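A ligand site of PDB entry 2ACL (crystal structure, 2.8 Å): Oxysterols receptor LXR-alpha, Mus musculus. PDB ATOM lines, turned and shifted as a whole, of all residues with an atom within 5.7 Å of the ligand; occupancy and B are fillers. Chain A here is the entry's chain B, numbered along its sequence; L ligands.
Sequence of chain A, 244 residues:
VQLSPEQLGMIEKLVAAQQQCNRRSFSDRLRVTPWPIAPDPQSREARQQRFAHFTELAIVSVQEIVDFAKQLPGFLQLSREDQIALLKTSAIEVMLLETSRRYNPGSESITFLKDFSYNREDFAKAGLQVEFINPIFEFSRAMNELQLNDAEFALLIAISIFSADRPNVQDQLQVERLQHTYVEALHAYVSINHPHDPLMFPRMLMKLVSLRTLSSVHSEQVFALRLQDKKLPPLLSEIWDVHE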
ATOM      1  N   PHE A  51      -6.894 -31.395  34.518  1.00  0.00           N
ATOM      2  CA  PHE A  51      -7.810 -31.900  33.511  1.00  0.00           C
ATOM      3  C   PHE A  51      -8.995 -32.609  34.165  1.00  0.00           C
ATOM      4  O   PHE A  51     -10.091 -32.651  33.616  1.00  0.00           O
ATOM      5  CB  PHE A  51      -7.078 -32.850  32.560  1.00  0.00           C
ATOM      6  CG  PHE A  51      -7.976 -33.561  31.595  1.00  0.00           C
ATOM      7  CD1 PHE A  51      -8.515 -34.797  31.917  1.00  0.00           C
ATOM      8  CD2 PHE A  51      -8.291 -32.998  30.375  1.00  0.00           C
ATOM      9  CE1 PHE A  51      -9.368 -35.462  31.023  1.00  0.00           C
ATOM     10  CE2 PHE A  51      -9.134 -33.644  29.487  1.00  0.00           C
ATOM     11  CZ  PHE A  51      -9.673 -34.880  29.808  1.00  0.00           C
ATOM     12  N   PHE A  54     -11.360 -29.578  35.469  1.00  0.00           N
ATOM     13  CA  PHE A  54     -12.174 -29.007  34.417  1.00  0.00           C
ATOM     14  C   PHE A  54     -13.240 -29.978  33.913  1.00  0.00           C
ATOM     15  O   PHE A  54     -14.411 -29.615  33.815  1.00  0.00           O
ATOM     16  CB  PHE A  54     -11.292 -28.566  33.241  1.00  0.00           C
ATOM     17  CG  PHE A  54     -11.199 -27.066  33.082  1.00  0.00           C
ATOM     18  CD1 PHE A  54     -10.624 -26.276  34.081  1.00  0.00           C
ATOM     19  CD2 PHE A  54     -11.678 -26.443  31.933  1.00  0.00           C
ATOM     20  CE1 PHE A  54     -10.525 -24.885  33.927  1.00  0.00           C
ATOM     21  CE2 PHE A  54     -11.587 -25.064  31.761  1.00  0.00           C
ATOM     22  CZ  PHE A  54     -11.004 -24.273  32.755  1.00  0.00           C
ATOM     23  N   THR A  55     -12.847 -31.208  33.586  1.00  0.00           N
ATOM     24  CA  THR A  55     -13.799 -32.194  33.084  1.00  0.00           C
ATOM     25  C   THR A  55     -14.909 -32.507  34.078  1.00  0.00           C
ATOM     26  O   THR A  55     -16.003 -32.904  33.683  1.00  0.00           O
ATOM     27  CB  THR A  55     -13.098 -33.537  32.724  1.00  0.00           C
ATOM     28  OG1 THR A  55     -12.183 -33.904  33.768  1.00  0.00           O
ATOM     29  CG2 THR A  55     -12.337 -33.422  31.413  1.00  0.00           C
ATOM     30  N   GLU A  56     -14.628 -32.339  35.363  1.00  0.00           N
ATOM     31  CA  GLU A  56     -15.631 -32.605  36.394  1.00  0.00           C
ATOM     32  C   GLU A  56     -16.639 -31.470  36.484  1.00  0.00           C
ATOM     33  O   GLU A  56     -17.851 -31.707  36.604  1.00  0.00           O
ATOM     34  CB  GLU A  56     -14.954 -32.847  37.746  1.00  0.00           C
ATOM     35  CG  GLU A  56     -14.206 -34.158  37.826  1.00  0.00           C
ATOM     36  CD  GLU A  56     -13.688 -34.476  39.221  1.00  0.00           C
ATOM     37  OE1 GLU A  56     -13.011 -35.526  39.368  1.00  0.00           O
ATOM     38  OE2 GLU A  56     -13.941 -33.686  40.161  1.00  0.00           O
ATOM     39  N   LEU A  57     -16.144 -30.225  36.466  1.00  0.00           N
ATOM     40  CA  LEU A  57     -17.006 -29.049  36.497  1.00  0.00           C
ATOM     41  C   LEU A  57     -17.903 -29.142  35.256  1.00  0.00           C
ATOM     42  O   LEU A  57     -19.055 -28.721  35.272  1.00  0.00           O
ATOM     43  CB  LEU A  57     -16.154 -27.781  36.463  1.00  0.00           C
ATOM     44  CG  LEU A  57     -15.395 -27.507  37.766  1.00  0.00           C
ATOM     45  CD1 LEU A  57     -14.531 -26.279  37.620  1.00  0.00           C
ATOM     46  CD2 LEU A  57     -16.376 -27.312  38.904  1.00  0.00           C
ATOM     47  N   ALA A  58     -17.359 -29.726  34.189  1.00  0.00           N
ATOM     48  CA  ALA A  58     -18.112 -29.920  32.966  1.00  0.00           C
ATOM     49  C   ALA A  58     -19.266 -30.891  33.234  1.00  0.00           C
ATOM     50  O   ALA A  58     -20.335 -30.797  32.629  1.00  0.00           O
ATOM     51  CB  ALA A  58     -17.200 -30.462  31.870  1.00  0.00           C
ATOM     52  N   SER A  61     -21.926 -29.289  35.391  1.00  0.00           N
ATOM     53  CA  SER A  61     -22.566 -28.391  34.463  1.00  0.00           C
ATOM     54  C   SER A  61     -23.650 -29.144  33.704  1.00  0.00           C
ATOM     55  O   SER A  61     -24.790 -28.706  33.649  1.00  0.00           O
ATOM     56  CB  SER A  61     -21.505 -27.835  33.505  1.00  0.00           C
ATOM     57  OG  SER A  61     -21.844 -26.526  33.056  1.00  0.00           O
ATOM     58  N   ILE A  92     -23.028 -27.759  25.043  1.00  0.00           N
ATOM     59  CA  ILE A  92     -21.854 -26.929  24.791  1.00  0.00           C
ATOM     60  C   ILE A  92     -22.152 -25.431  24.795  1.00  0.00           C
ATOM     61  O   ILE A  92     -21.410 -24.637  25.385  1.00  0.00           O
ATOM     62  CB  ILE A  92     -21.203 -27.294  23.458  1.00  0.00           C
ATOM     63  CG1 ILE A  92     -19.886 -26.534  23.291  1.00  0.00           C
ATOM     64  CG2 ILE A  92     -22.158 -26.967  22.314  1.00  0.00           C
ATOM     65  CD1 ILE A  92     -18.911 -26.718  24.448  1.00  0.00           C
ATOM     66  N   MET A  95     -22.979 -24.095  28.143  1.00  0.00           N
ATOM     67  CA  MET A  95     -21.757 -24.005  28.935  1.00  0.00           C
ATOM     68  C   MET A  95     -21.023 -22.706  28.606  1.00  0.00           C
ATOM     69  O   MET A  95     -20.615 -21.975  29.504  1.00  0.00           O
ATOM     70  CB  MET A  95     -20.837 -25.212  28.674  1.00  0.00           C
ATOM     71  CG  MET A  95     -21.184 -26.461  29.477  1.00  0.00           C
ATOM     72  SD  MET A  95     -20.151 -27.939  29.094  1.00  0.00           S
ATOM     73  CE  MET A  95     -21.399 -29.192  28.666  1.00  0.00           C
ATOM     74  N   LEU A  96     -20.870 -22.419  27.314  1.00  0.00           N
ATOM     75  CA  LEU A  96     -20.187 -21.207  26.905  1.00  0.00           C
ATOM     76  C   LEU A  96     -20.951 -20.007  27.417  1.00  0.00           C
ATOM     77  O   LEU A  96     -20.356 -19.024  27.864  1.00  0.00           O
ATOM     78  CB  LEU A  96     -20.064 -21.167  25.388  1.00  0.00           C
ATOM     79  CG  LEU A  96     -18.955 -22.067  24.816  1.00  0.00           C
ATOM     80  CD1 LEU A  96     -19.190 -22.342  23.329  1.00  0.00           C
ATOM     81  CD2 LEU A  96     -17.620 -21.373  25.041  1.00  0.00           C
ATOM     82  N   GLU A  98     -22.927 -19.917  30.131  1.00  0.00           N
ATOM     83  CA  GLU A  98     -22.733 -19.804  31.564  1.00  0.00           C
ATOM     84  C   GLU A  98     -21.307 -19.439  31.921  1.00  0.00           C
ATOM     85  O   GLU A  98     -21.014 -19.156  33.075  1.00  0.00           O
ATOM     86  CB  GLU A  98     -23.125 -21.097  32.255  1.00  0.00           C
ATOM     87  CG  GLU A  98     -24.640 -21.262  32.360  1.00  0.00           C
ATOM     88  CD  GLU A  98     -25.157 -21.141  33.793  1.00  0.00           C
ATOM     89  OE1 GLU A  98     -24.571 -20.360  34.572  1.00  0.00           O
ATOM     90  OE2 GLU A  98     -26.156 -21.844  34.129  1.00  0.00           O
ATOM     91  N   THR A  99     -20.426 -19.423  30.941  1.00  0.00           N
ATOM     92  CA  THR A  99     -19.044 -19.084  31.197  1.00  0.00           C
ATOM     93  C   THR A  99     -18.919 -17.585  31.129  1.00  0.00           C
ATOM     94  O   THR A  99     -18.348 -16.952  32.019  1.00  0.00           O
ATOM     95  CB  THR A  99     -18.114 -19.709  30.173  1.00  0.00           C
ATOM     96  OG1 THR A  99     -18.433 -21.101  30.048  1.00  0.00           O
ATOM     97  CG2 THR A  99     -16.676 -19.582  30.629  1.00  0.00           C
ATOM     98  N   ARG A 102     -19.902 -15.606  34.036  1.00  0.00           N
ATOM     99  CA  ARG A 102     -18.909 -15.587  35.090  1.00  0.00           C
ATOM    100  C   ARG A 102     -17.578 -14.971  34.634  1.00  0.00           C
ATOM    101  O   ARG A 102     -16.557 -15.137  35.270  1.00  0.00           O
ATOM    102  CB  ARG A 102     -18.687 -17.010  35.596  1.00  0.00           C
ATOM    103  CG  ARG A 102     -19.966 -17.691  36.052  1.00  0.00           C
ATOM    104  CD  ARG A 102     -19.697 -19.127  36.511  1.00  0.00           C
ATOM    105  NE  ARG A 102     -20.790 -19.634  37.338  1.00  0.00           N
ATOM    106  CZ  ARG A 102     -22.002 -19.935  36.887  1.00  0.00           C
ATOM    107  NH1 ARG A 102     -22.299 -19.777  35.612  1.00  0.00           N
ATOM    108  NH2 ARG A 102     -22.930 -20.371  37.737  1.00  0.00           N
ATOM    109  N   PHE A 112     -15.491 -20.167  38.046  1.00  0.00           N
ATOM    110  CA  PHE A 112     -16.480 -21.236  38.054  1.00  0.00           C
ATOM    111  C   PHE A 112     -16.981 -21.593  39.455  1.00  0.00           C
ATOM    112  O   PHE A 112     -16.201 -21.649  40.405  1.00  0.00           O
ATOM    113  CB  PHE A 112     -15.894 -22.475  37.393  1.00  0.00           C
ATOM    114  CG  PHE A 112     -15.611 -22.293  35.938  1.00  0.00           C
ATOM    115  CD1 PHE A 112     -16.623 -21.936  35.064  1.00  0.00           C
ATOM    116  CD2 PHE A 112     -14.330 -22.476  35.448  1.00  0.00           C
ATOM    117  CE1 PHE A 112     -16.369 -21.767  33.712  1.00  0.00           C
ATOM    118  CE2 PHE A 112     -14.055 -22.307  34.093  1.00  0.00           C
ATOM    119  CZ  PHE A 112     -15.083 -21.954  33.230  1.00  0.00           C
ATOM    120  N   PHE A 123      -6.749 -22.244  31.731  1.00  0.00           N
ATOM    121  CA  PHE A 123      -7.472 -23.006  30.737  1.00  0.00           C
ATOM    122  C   PHE A 123      -6.483 -23.913  30.007  1.00  0.00           C
ATOM    123  O   PHE A 123      -6.730 -25.093  29.830  1.00  0.00           O
ATOM    124  CB  PHE A 123      -8.191 -22.056  29.778  1.00  0.00           C
ATOM    125  CG  PHE A 123      -9.666 -21.936  30.025  1.00  0.00           C
ATOM    126  CD1 PHE A 123     -10.587 -22.550  29.178  1.00  0.00           C
ATOM    127  CD2 PHE A 123     -10.140 -21.226  31.141  1.00  0.00           C
ATOM    128  CE1 PHE A 123     -11.949 -22.446  29.426  1.00  0.00           C
ATOM    129  CE2 PHE A 123     -11.501 -21.122  31.390  1.00  0.00           C
ATOM    130  CZ  PHE A 123     -12.411 -21.727  30.526  1.00  0.00           C
ATOM    131  N   ALA A 126      -5.117 -26.835  31.666  1.00  0.00           N
ATOM    132  CA  ALA A 126      -6.096 -27.886  31.854  1.00  0.00           C
ATOM    133  C   ALA A 126      -6.360 -28.800  30.666  1.00  0.00           C
ATOM    134  O   ALA A 126      -7.232 -29.672  30.750  1.00  0.00           O
ATOM    135  CB  ALA A 126      -7.388 -27.286  32.357  1.00  0.00           C
ATOM    136  N   GLY A 127      -5.639 -28.642  29.562  1.00  0.00           N
ATOM    137  CA  GLY A 127      -5.869 -29.530  28.440  1.00  0.00           C
ATOM    138  C   GLY A 127      -6.409 -28.871  27.188  1.00  0.00           C
ATOM    139  O   GLY A 127      -6.158 -29.354  26.074  1.00  0.00           O
ATOM    140  N   LEU A 128      -7.176 -27.790  27.354  1.00  0.00           N
ATOM    141  CA  LEU A 128      -7.740 -27.073  26.222  1.00  0.00           C
ATOM    142  C   LEU A 128      -6.617 -26.506  25.369  1.00  0.00           C
ATOM    143  O   LEU A 128      -5.481 -26.356  25.832  1.00  0.00           O
ATOM    144  CB  LEU A 128      -8.638 -25.914  26.694  1.00  0.00           C
ATOM    145  CG  LEU A 128      -9.967 -26.230  27.391  1.00  0.00           C
ATOM    146  CD1 LEU A 128     -10.782 -27.185  26.539  1.00  0.00           C
ATOM    147  CD2 LEU A 128      -9.699 -26.836  28.750  1.00  0.00           C
ATOM    148  N   PHE A 132      -9.131 -22.650  20.959  1.00  0.00           N
ATOM    149  CA  PHE A 132     -10.473 -22.773  21.498  1.00  0.00           C
ATOM    150  C   PHE A 132     -10.618 -21.844  22.671  1.00  0.00           C
ATOM    151  O   PHE A 132     -11.699 -21.327  22.918  1.00  0.00           O
ATOM    152  CB  PHE A 132     -10.754 -24.202  21.946  1.00  0.00           C
ATOM    153  CG  PHE A 132     -12.095 -24.364  22.588  1.00  0.00           C
ATOM    154  CD1 PHE A 132     -13.210 -23.717  22.091  1.00  0.00           C
ATOM    155  CD2 PHE A 132     -12.259 -25.227  23.667  1.00  0.00           C
ATOM    156  CE1 PHE A 132     -14.468 -23.925  22.635  1.00  0.00           C
ATOM    157  CE2 PHE A 132     -13.522 -25.450  24.218  1.00  0.00           C
ATOM    158  CZ  PHE A 132     -14.626 -24.794  23.704  1.00  0.00           C
ATOM    159  N   ILE A 136     -13.151 -18.536  23.151  1.00  0.00           N
ATOM    160  CA  ILE A 136     -13.937 -18.610  24.380  1.00  0.00           C
ATOM    161  C   ILE A 136     -13.890 -17.282  25.129  1.00  0.00           C
ATOM    162  O   ILE A 136     -14.928 -16.679  25.403  1.00  0.00           O
ATOM    163  CB  ILE A 136     -13.434 -19.745  25.321  1.00  0.00           C
ATOM    164  CG1 ILE A 136     -13.932 -21.099  24.824  1.00  0.00           C
ATOM    165  CG2 ILE A 136     -13.891 -19.506  26.761  1.00  0.00           C
ATOM    166  CD1 ILE A 136     -13.401 -22.296  25.611  1.00  0.00           C
ATOM    167  N   HIS A 218     -15.121 -26.310  19.288  1.00  0.00           N
ATOM    168  CA  HIS A 218     -15.040 -27.183  20.429  1.00  0.00           C
ATOM    169  C   HIS A 218     -14.994 -28.634  19.957  1.00  0.00           C
ATOM    170  O   HIS A 218     -14.231 -29.450  20.495  1.00  0.00           O
ATOM    171  CB  HIS A 218     -16.245 -26.938  21.340  1.00  0.00           C
ATOM    172  CG  HIS A 218     -16.481 -28.021  22.350  1.00  0.00           C
ATOM    173  ND1 HIS A 218     -17.391 -29.037  22.158  1.00  0.00           N
ATOM    174  CD2 HIS A 218     -15.911 -28.233  23.560  1.00  0.00           C
ATOM    175  CE1 HIS A 218     -17.385 -29.825  23.214  1.00  0.00           C
ATOM    176  NE2 HIS A 218     -16.498 -29.370  24.077  1.00  0.00           N
ATOM    177  N   GLN A 221     -11.871 -29.614  19.075  1.00  0.00           N
ATOM    178  CA  GLN A 221     -11.070 -29.804  20.278  1.00  0.00           C
ATOM    179  C   GLN A 221     -11.312 -31.164  20.934  1.00  0.00           C
ATOM    180  O   GLN A 221     -10.526 -31.613  21.774  1.00  0.00           O
ATOM    181  CB  GLN A 221     -11.351 -28.658  21.260  1.00  0.00           C
ATOM    182  CG  GLN A 221     -10.880 -28.868  22.681  1.00  0.00           C
ATOM    183  CD  GLN A 221      -9.384 -28.715  22.831  1.00  0.00           C
ATOM    184  OE1 GLN A 221      -8.900 -27.642  23.212  1.00  0.00           O
ATOM    185  NE2 GLN A 221      -8.644 -29.790  22.545  1.00  0.00           N
ATOM    186  N   VAL A 222     -12.409 -31.813  20.566  1.00  0.00           N
ATOM    187  CA  VAL A 222     -12.686 -33.114  21.131  1.00  0.00           C
ATOM    188  C   VAL A 222     -11.877 -34.116  20.344  1.00  0.00           C
ATOM    189  O   VAL A 222     -11.279 -35.040  20.921  1.00  0.00           O
ATOM    190  CB  VAL A 222     -14.180 -33.496  21.065  1.00  0.00           C
ATOM    191  CG1 VAL A 222     -14.353 -34.973  21.377  1.00  0.00           C
ATOM    192  CG2 VAL A 222     -14.968 -32.704  22.094  1.00  0.00           C
ATOM    193  N   LEU A 225      -8.261 -34.663  21.003  1.00  0.00           N
ATOM    194  CA  LEU A 225      -7.951 -35.523  22.132  1.00  0.00           C
ATOM    195  C   LEU A 225      -7.474 -36.893  21.670  1.00  0.00           C
ATOM    196  O   LEU A 225      -6.595 -37.491  22.271  1.00  0.00           O
ATOM    197  CB  LEU A 225      -9.178 -35.675  23.042  1.00  0.00           C
ATOM    198  CG  LEU A 225      -9.438 -34.557  24.046  1.00  0.00           C
ATOM    199  CD1 LEU A 225     -10.484 -35.013  25.048  1.00  0.00           C
ATOM    200  CD2 LEU A 225      -8.161 -34.203  24.761  1.00  0.00           C
ATOM    201  N   LEU A 232     -12.028 -38.541  28.131  1.00  0.00           N
ATOM    202  CA  LEU A 232     -13.142 -37.778  28.697  1.00  0.00           C
ATOM    203  C   LEU A 232     -13.896 -38.777  29.563  1.00  0.00           C
ATOM    204  O   LEU A 232     -14.007 -39.956  29.219  1.00  0.00           O
ATOM    205  CB  LEU A 232     -14.057 -37.231  27.589  1.00  0.00           C
ATOM    206  CG  LEU A 232     -13.534 -36.054  26.770  1.00  0.00           C
ATOM    207  CD1 LEU A 232     -14.587 -35.631  25.759  1.00  0.00           C
ATOM    208  CD2 LEU A 232     -13.163 -34.892  27.685  1.00  0.00           C
ATOM    209  N   LEU A 236     -19.264 -37.013  29.554  1.00  0.00           N
ATOM    210  CA  LEU A 236     -18.850 -36.117  28.504  1.00  0.00           C
ATOM    211  C   LEU A 236     -18.626 -36.906  27.222  1.00  0.00           C
ATOM    212  O   LEU A 236     -19.086 -36.491  26.157  1.00  0.00           O
ATOM    213  CB  LEU A 236     -17.594 -35.334  28.928  1.00  0.00           C
ATOM    214  CG  LEU A 236     -17.855 -34.521  30.198  1.00  0.00           C
ATOM    215  CD1 LEU A 236     -16.660 -33.675  30.570  1.00  0.00           C
ATOM    216  CD2 LEU A 236     -19.076 -33.640  29.996  1.00  0.00           C
ATOM    217  N   TRP A 240     -20.611 -36.065  23.621  1.00  0.00           N
ATOM    218  CA  TRP A 240     -19.791 -35.502  22.567  1.00  0.00           C
ATOM    219  C   TRP A 240     -19.310 -36.561  21.576  1.00  0.00           C
ATOM    220  O   TRP A 240     -19.904 -36.698  20.517  1.00  0.00           O
ATOM    221  CB  TRP A 240     -18.649 -34.676  23.157  1.00  0.00           C
ATOM    222  CG  TRP A 240     -19.180 -33.419  23.816  1.00  0.00           C
ATOM    223  CD1 TRP A 240     -20.292 -32.711  23.449  1.00  0.00           C
ATOM    224  CD2 TRP A 240     -18.616 -32.716  24.938  1.00  0.00           C
ATOM    225  NE1 TRP A 240     -20.455 -31.622  24.267  1.00  0.00           N
ATOM    226  CE2 TRP A 240     -19.445 -31.598  25.194  1.00  0.00           C
ATOM    227  CE3 TRP A 240     -17.495 -32.924  25.757  1.00  0.00           C
ATOM    228  CZ2 TRP A 240     -19.184 -30.691  26.219  1.00  0.00           C
ATOM    229  CZ3 TRP A 240     -17.242 -32.018  26.787  1.00  0.00           C
ATOM    230  CH2 TRP A 240     -18.083 -30.909  27.002  1.00  0.00           C
HETATM  231  C1  LIG L   1     -19.642 -23.439  32.909  1.00  0.00           C
HETATM  232  O1  LIG L   1     -19.221 -24.614  33.623  1.00  0.00           O
HETATM  233  C2  LIG L   1     -18.131 -25.299  33.089  1.00  0.00           C
HETATM  234  C3  LIG L   1     -18.441 -26.192  32.011  1.00  0.00           C
HETATM  235  C4  LIG L   1     -17.414 -26.943  31.405  1.00  0.00           C
HETATM  236  C5  LIG L   1     -16.056 -26.830  31.842  1.00  0.00           C
HETATM  237  N1  LIG L   1     -14.970 -27.559  31.264  1.00  0.00           N
HETATM  238  C6  LIG L   1     -14.751 -28.050  29.979  1.00  0.00           C
HETATM  239  C7  LIG L   1     -14.962 -27.477  28.757  1.00  0.00           C
HETATM  240  C8  LIG L   1     -14.550 -28.445  27.710  1.00  0.00           C
HETATM  241  O2  LIG L   1     -14.606 -28.237  26.514  1.00  0.00           O
HETATM  242  N2  LIG L   1     -14.100 -29.561  28.341  1.00  0.00           N
HETATM  243  C9  LIG L   1     -13.603 -30.758  27.649  1.00  0.00           C
HETATM  244  C10 LIG L   1     -12.117 -30.755  27.334  1.00  0.00           C
HETATM  245  C11 LIG L   1     -11.663 -31.077  26.012  1.00  0.00           C
HETATM  246  C12 LIG L   1     -10.278 -31.079  25.687  1.00  0.00           C
HETATM  247  C13 LIG L   1      -9.320 -30.764  26.687  1.00  0.00           C
HETATM  248  C14 LIG L   1      -9.747 -30.447  28.012  1.00  0.00           C
HETATM  249  C15 LIG L   1     -11.137 -30.440  28.331  1.00  0.00           C
HETATM  250  C16 LIG L   1     -14.188 -29.422  29.695  1.00  0.00           C
HETATM  251  O3  LIG L   1     -13.865 -30.255  30.526  1.00  0.00           O
HETATM  252  C17 LIG L   1     -15.507 -26.137  28.493  1.00  0.00           C
HETATM  253  C18 LIG L   1     -14.955 -24.974  29.118  1.00  0.00           C
HETATM  254  C19 LIG L   1     -15.498 -23.693  28.853  1.00  0.00           C
HETATM  255  C20 LIG L   1     -16.587 -23.551  27.961  1.00  0.00           C
HETATM  256  C21 LIG L   1     -17.156 -24.689  27.338  1.00  0.00           C
HETATM  257  C22 LIG L   1     -16.614 -25.978  27.598  1.00  0.00           C
HETATM  258  C23 LIG L   1     -15.761 -25.943  32.913  1.00  0.00           C
HETATM  259  C24 LIG L   1     -16.789 -25.181  33.541  1.00  0.00           C
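O3 of the ligand sits close to N of Thr 55 (3.4 Å).
A ring nitrogen (NE2) of His 218 sits close to an oxygen (O2) of the ligand (3.3 Å).
OG of Ser 61 sits at hydrogen-bond distance from O1 of the ligand (3.3 Å).
O of Phe 54 is in hydrogen-bond range of N1 of the ligand (3.3 Å).
Merely in contact with the ligand: Phe 51 (3.6 Å), Leu 57 (3.96 Å), Ala 58 (3.4 Å), Ile 92 (3.9 Å), Met 95 (3.7 Å), Leu 96 (3.8 Å), Thr 99 (3.7 Å), Phe 112 (3.4 Å), Phe 123 (3.8 Å), Ala 126 (3.8 Å), Gly 127 (3.5 Å), Leu 128 (3.7 Å), Phe 132 (3.8 Å), Gln 221 (3.8 Å), Leu 225 (3.9 Å) and Trp 240 (3.9 Å).
Hydrophobic or aromatic side chains within 4 Å of the ligand: Phe 51, Phe 54, Leu 57, Ala 58, Ile 92, Met 95, Leu 96, Phe 112, Phe 123, Leu 128, Phe 132, His 218, Leu 225 and Trp 240.
Within 4 Å of the ligand: Phe 51, Phe 54, Thr 55, Leu 57, Ala 58, Ser 61, Ile 92, Met 95, Leu 96, Thr 99, Phe 112, Phe 123, Ala 126, Gly 127, Leu 128, Phe 132, His 218, Gln 221, Leu 225 and Trp 240.
The nearest printed residue that does not touch the ligand is Ile 136 (4.1 Å).
OG1 of Thr 55 sits at hydrogen-bond distance from O of Phe 51 (2.4 Å).
OG1 of Thr 99 sits at hydrogen-bond distance from O of Met 95, 2.4 Å away.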
